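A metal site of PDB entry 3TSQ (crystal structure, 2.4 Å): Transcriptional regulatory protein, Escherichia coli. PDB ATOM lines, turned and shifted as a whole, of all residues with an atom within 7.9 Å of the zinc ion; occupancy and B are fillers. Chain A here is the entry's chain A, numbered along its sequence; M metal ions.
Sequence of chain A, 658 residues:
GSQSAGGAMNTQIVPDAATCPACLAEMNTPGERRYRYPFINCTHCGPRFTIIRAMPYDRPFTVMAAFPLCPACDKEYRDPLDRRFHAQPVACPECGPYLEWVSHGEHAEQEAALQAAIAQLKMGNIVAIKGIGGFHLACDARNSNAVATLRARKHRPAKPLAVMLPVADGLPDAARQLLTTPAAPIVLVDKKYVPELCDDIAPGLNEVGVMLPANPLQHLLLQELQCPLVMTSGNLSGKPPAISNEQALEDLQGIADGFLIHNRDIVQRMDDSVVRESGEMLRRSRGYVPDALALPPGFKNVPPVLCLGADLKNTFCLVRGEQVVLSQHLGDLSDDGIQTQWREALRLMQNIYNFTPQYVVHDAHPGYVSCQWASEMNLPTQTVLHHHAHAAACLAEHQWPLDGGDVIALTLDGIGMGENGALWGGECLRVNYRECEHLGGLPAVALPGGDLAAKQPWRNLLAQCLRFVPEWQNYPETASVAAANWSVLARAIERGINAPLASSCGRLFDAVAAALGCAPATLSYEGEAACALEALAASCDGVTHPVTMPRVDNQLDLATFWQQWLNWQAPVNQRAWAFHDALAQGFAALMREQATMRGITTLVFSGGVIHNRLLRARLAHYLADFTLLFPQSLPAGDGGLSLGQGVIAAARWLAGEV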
ATOM      1  N   ALA A  17      11.384   5.175  24.612  1.00  0.00           N
ATOM      2  CA  ALA A  17      12.579   4.651  23.988  1.00  0.00           C
ATOM      3  C   ALA A  17      12.296   4.169  22.586  1.00  0.00           C
ATOM      4  O   ALA A  17      11.317   3.474  22.355  1.00  0.00           O
ATOM      5  CB  ALA A  17      13.230   3.531  24.838  1.00  0.00           C
ATOM      6  N   ALA A  18      13.191   4.527  21.647  1.00  0.00           N
ATOM      7  CA  ALA A  18      13.107   4.054  20.267  1.00  0.00           C
ATOM      8  C   ALA A  18      13.008   2.528  20.258  1.00  0.00           C
ATOM      9  O   ALA A  18      13.712   1.906  21.055  1.00  0.00           O
ATOM     10  CB  ALA A  18      14.349   4.482  19.538  1.00  0.00           C
ATOM     11  N   THR A  19      12.188   1.925  19.370  1.00  0.00           N
ATOM     12  CA  THR A  19      12.196   0.472  19.135  1.00  0.00           C
ATOM     13  C   THR A  19      13.644  -0.135  19.038  1.00  0.00           C
ATOM     14  O   THR A  19      14.500   0.385  18.307  1.00  0.00           O
ATOM     15  CB  THR A  19      11.392   0.178  17.862  1.00  0.00           C
ATOM     16  OG1 THR A  19      10.116   0.828  17.988  1.00  0.00           O
ATOM     17  CG2 THR A  19      11.178  -1.391  17.607  1.00  0.00           C
ATOM     18  N   CYS A  20      13.917  -1.214  19.790  1.00  0.00           N
ATOM     19  CA  CYS A  20      15.283  -1.788  19.859  1.00  0.00           C
ATOM     20  C   CYS A  20      15.599  -2.751  18.699  1.00  0.00           C
ATOM     21  O   CYS A  20      14.682  -3.197  17.995  1.00  0.00           O
ATOM     22  CB  CYS A  20      15.500  -2.454  21.210  1.00  0.00           C
ATOM     23  SG  CYS A  20      14.665  -4.101  21.386  1.00  0.00           S
ATOM     24  N   PRO A  21      16.894  -3.093  18.465  1.00  0.00           N
ATOM     25  CA  PRO A  21      17.159  -4.069  17.355  1.00  0.00           C
ATOM     26  C   PRO A  21      16.375  -5.377  17.451  1.00  0.00           C
ATOM     27  O   PRO A  21      15.787  -5.813  16.474  1.00  0.00           O
ATOM     28  CB  PRO A  21      18.674  -4.316  17.422  1.00  0.00           C
ATOM     29  CG  PRO A  21      19.215  -3.055  18.092  1.00  0.00           C
ATOM     30  CD  PRO A  21      18.144  -2.658  19.118  1.00  0.00           C
ATOM     31  N   ALA A  22      16.328  -5.984  18.621  1.00  0.00           N
ATOM     32  CA  ALA A  22      15.606  -7.265  18.820  1.00  0.00           C
ATOM     33  C   ALA A  22      14.080  -7.213  18.507  1.00  0.00           C
ATOM     34  O   ALA A  22      13.532  -8.169  18.000  1.00  0.00           O
ATOM     35  CB  ALA A  22      15.869  -7.816  20.222  1.00  0.00           C
ATOM     36  N   CYS A  23      13.405  -6.117  18.821  1.00  0.00           N
ATOM     37  CA  CYS A  23      11.994  -6.010  18.496  1.00  0.00           C
ATOM     38  C   CYS A  23      11.844  -5.787  16.984  1.00  0.00           C
ATOM     39  O   CYS A  23      10.993  -6.387  16.354  1.00  0.00           O
ATOM     40  CB  CYS A  23      11.323  -4.856  19.248  1.00  0.00           C
ATOM     41  SG  CYS A  23      10.914  -5.271  20.963  1.00  0.00           S
ATOM     42  N   LEU A  24      12.673  -4.908  16.422  1.00  0.00           N
ATOM     43  CA  LEU A  24      12.767  -4.711  14.983  1.00  0.00           C
ATOM     44  C   LEU A  24      12.978  -6.013  14.207  1.00  0.00           C
ATOM     45  O   LEU A  24      12.228  -6.306  13.276  1.00  0.00           O
ATOM     46  CB  LEU A  24      13.841  -3.675  14.635  1.00  0.00           C
ATOM     47  CG  LEU A  24      13.650  -3.164  13.202  1.00  0.00           C
ATOM     48  CD1 LEU A  24      12.310  -2.415  13.119  1.00  0.00           C
ATOM     49  CD2 LEU A  24      14.845  -2.280  12.648  1.00  0.00           C
ATOM     50  N   GLU A  26      12.251  -9.013  15.396  1.00  0.00           N
ATOM     51  CA  GLU A  26      11.058  -9.848  15.571  1.00  0.00           C
ATOM     52  C   GLU A  26       9.902  -9.418  14.633  1.00  0.00           C
ATOM     53  O   GLU A  26       9.192 -10.260  14.080  1.00  0.00           O
ATOM     54  CB  GLU A  26      10.649  -9.856  17.042  1.00  0.00           C
ATOM     55  CG  GLU A  26       9.363 -10.597  17.421  1.00  0.00           C
ATOM     56  CD  GLU A  26       9.008 -10.428  18.920  1.00  0.00           C
ATOM     57  OE1 GLU A  26       9.880  -9.948  19.716  1.00  0.00           O
ATOM     58  OE2 GLU A  26       7.853 -10.735  19.306  1.00  0.00           O
ATOM     59  N   ILE A  40       4.654  -3.608  18.643  1.00  0.00           N
ATOM     60  CA  ILE A  40       5.676  -4.387  19.299  1.00  0.00           C
ATOM     61  C   ILE A  40       6.552  -3.480  20.218  1.00  0.00           C
ATOM     62  O   ILE A  40       6.987  -2.399  19.791  1.00  0.00           O
ATOM     63  CB  ILE A  40       6.508  -5.153  18.246  1.00  0.00           C
ATOM     64  CG1 ILE A  40       7.516  -6.118  18.883  1.00  0.00           C
ATOM     65  CG2 ILE A  40       7.229  -4.195  17.288  1.00  0.00           C
ATOM     66  CD1 ILE A  40       8.107  -7.111  17.825  1.00  0.00           C
ATOM     67  N   ASN A  41       6.743  -3.916  21.484  1.00  0.00           N
ATOM     68  CA  ASN A  41       7.720  -3.321  22.424  1.00  0.00           C
ATOM     69  C   ASN A  41       8.209  -4.406  23.346  1.00  0.00           C
ATOM     70  O   ASN A  41       7.659  -5.497  23.333  1.00  0.00           O
ATOM     71  CB  ASN A  41       7.154  -2.156  23.252  1.00  0.00           C
ATOM     72  CG  ASN A  41       5.871  -2.517  23.990  1.00  0.00           C
ATOM     73  OD1 ASN A  41       4.774  -2.271  23.483  1.00  0.00           O
ATOM     74  ND2 ASN A  41       5.991  -3.093  25.194  1.00  0.00           N
ATOM     75  N   CYS A  42       9.227  -4.126  24.140  1.00  0.00           N
ATOM     76  CA  CYS A  42       9.698  -5.070  25.120  1.00  0.00           C
ATOM     77  C   CYS A  42      10.197  -4.293  26.333  1.00  0.00           C
ATOM     78  O   CYS A  42       9.938  -3.118  26.503  1.00  0.00           O
ATOM     79  CB  CYS A  42      10.815  -5.975  24.559  1.00  0.00           C
ATOM     80  SG  CYS A  42      12.428  -5.103  24.351  1.00  0.00           S
ATOM     81  N   THR A  43      10.938  -4.981  27.178  1.00  0.00           N
ATOM     82  CA  THR A  43      11.352  -4.423  28.452  1.00  0.00           C
ATOM     83  C   THR A  43      12.332  -3.281  28.250  1.00  0.00           C
ATOM     84  O   THR A  43      12.428  -2.409  29.093  1.00  0.00           O
ATOM     85  CB  THR A  43      11.945  -5.541  29.400  1.00  0.00           C
ATOM     86  OG1 THR A  43      11.935  -5.054  30.743  1.00  0.00           O
ATOM     87  CG2 THR A  43      13.363  -5.947  29.013  1.00  0.00           C
ATOM     88  N   HIS A  44      13.029  -3.308  27.113  1.00  0.00           N
ATOM     89  CA  HIS A  44      14.045  -2.310  26.743  1.00  0.00           C
ATOM     90  C   HIS A  44      13.568  -1.167  25.833  1.00  0.00           C
ATOM     91  O   HIS A  44      14.337  -0.267  25.602  1.00  0.00           O
ATOM     92  CB  HIS A  44      15.251  -3.005  26.084  1.00  0.00           C
ATOM     93  CG  HIS A  44      15.884  -4.018  26.968  1.00  0.00           C
ATOM     94  ND1 HIS A  44      15.859  -5.377  26.696  1.00  0.00           N
ATOM     95  CD2 HIS A  44      16.451  -3.893  28.195  1.00  0.00           C
ATOM     96  CE1 HIS A  44      16.450  -6.035  27.679  1.00  0.00           C
ATOM     97  NE2 HIS A  44      16.808  -5.161  28.601  1.00  0.00           N
ATOM     98  N   CYS A  45      12.357  -1.188  25.272  1.00  0.00           N
ATOM     99  CA  CYS A  45      12.006  -0.151  24.319  1.00  0.00           C
ATOM    100  C   CYS A  45      10.496   0.138  24.365  1.00  0.00           C
ATOM    101  O   CYS A  45       9.757  -0.596  25.025  1.00  0.00           O
ATOM    102  CB  CYS A  45      12.466  -0.526  22.900  1.00  0.00           C
ATOM    103  SG  CYS A  45      11.354  -1.668  22.081  1.00  0.00           S
ATOM    104  N   GLY A  46      10.034   1.175  23.670  1.00  0.00           N
ATOM    105  CA  GLY A  46       8.618   1.460  23.613  1.00  0.00           C
ATOM    106  C   GLY A  46       8.268   2.701  24.398  1.00  0.00           C
ATOM    107  O   GLY A  46       9.136   3.327  24.986  1.00  0.00           O
ATOM    108  N   ARG A  48       6.753   5.194  27.296  1.00  0.00           N
ATOM    109  CA  ARG A  48       6.777   5.074  28.778  1.00  0.00           C
ATOM    110  C   ARG A  48       5.913   6.166  29.388  1.00  0.00           C
ATOM    111  O   ARG A  48       4.749   5.967  29.695  1.00  0.00           O
ATOM    112  CB  ARG A  48       8.234   5.116  29.344  1.00  0.00           C
ATOM    113  CG  ARG A  48       9.143   3.946  28.951  1.00  0.00           C
ATOM    114  CD  ARG A  48       8.690   2.615  29.613  1.00  0.00           C
ATOM    115  NE  ARG A  48       9.598   1.512  29.240  1.00  0.00           N
ATOM    116  CZ  ARG A  48       9.376   0.646  28.255  1.00  0.00           C
ATOM    117  NH1 ARG A  48      10.266  -0.279  27.988  1.00  0.00           N
ATOM    118  NH2 ARG A  48       8.260   0.701  27.522  1.00  0.00           N
ATOM    119  N   ARG A  83      12.564 -11.446  27.107  1.00  0.00           N
ATOM    120  CA  ARG A  83      12.816 -10.032  26.798  1.00  0.00           C
ATOM    121  C   ARG A  83      11.641  -9.083  27.124  1.00  0.00           C
ATOM    122  O   ARG A  83      11.842  -7.862  27.251  1.00  0.00           O
ATOM    123  CB  ARG A  83      13.247  -9.842  25.324  1.00  0.00           C
ATOM    124  CG  ARG A  83      13.934  -8.475  25.083  1.00  0.00           C
ATOM    125  CD  ARG A  83      14.427  -8.261  23.665  1.00  0.00           C
ATOM    126  NE  ARG A  83      13.365  -7.948  22.720  1.00  0.00           N
ATOM    127  CZ  ARG A  83      12.728  -8.854  21.974  1.00  0.00           C
ATOM    128  NH1 ARG A  83      13.011 -10.133  22.095  1.00  0.00           N
ATOM    129  NH2 ARG A  83      11.779  -8.507  21.129  1.00  0.00           N
ATOM    130  N   ARG A  84      10.438  -9.658  27.243  1.00  0.00           N
ATOM    131  CA  ARG A  84       9.191  -8.925  27.508  1.00  0.00           C
ATOM    132  C   ARG A  84       8.669  -9.158  28.928  1.00  0.00           C
ATOM    133  O   ARG A  84       7.486  -8.894  29.213  1.00  0.00           O
ATOM    134  CB  ARG A  84       8.115  -9.302  26.483  1.00  0.00           C
ATOM    135  CG  ARG A  84       8.537  -9.006  25.073  1.00  0.00           C
ATOM    136  CD  ARG A  84       7.797  -9.799  24.039  1.00  0.00           C
ATOM    137  NE  ARG A  84       8.751 -10.449  23.118  1.00  0.00           N
ATOM    138  CZ  ARG A  84       9.180 -11.721  23.229  1.00  0.00           C
ATOM    139  NH1 ARG A  84       8.741 -12.508  24.213  1.00  0.00           N
ATOM    140  NH2 ARG A  84      10.029 -12.200  22.349  1.00  0.00           N
HETATM  141 ZN    ZN M   1      12.308  -3.894  22.257  1.00  0.00          ZN
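NH2 of Arg 83 lies close to SG of Cys 23 (3.4 Å).
The backbone carbonyl oxygen of Cys 42 sits at hydrogen-bond distance from the guanidinium group of Arg 48 (3.2 Å).
SG of Cys 42 sits close to N of His 44, 3.3 Å away.
SG of Cys 42 sits close to NE of Arg 83 (3.4 Å).
The guanidinium group (NH1) of Arg 48 lies within hydrogen-bond range of the backbone carbonyl oxygen (O) of Cys 45 (3.0 Å).
N of Ala 22 sits close to SG of Cys 20, 3.7 Å away.
The zinc ion is bound by the side-chain sulfur of Cys 23 (2.3 Å), the side-chain sulfur of Cys 42 (2.4 Å), the side-chain sulfur of Cys 45 (2.4 Å) and the side-chain sulfur of Cys 20 (2.5 Å).
The zinc ion has four donor atoms within binding distance.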
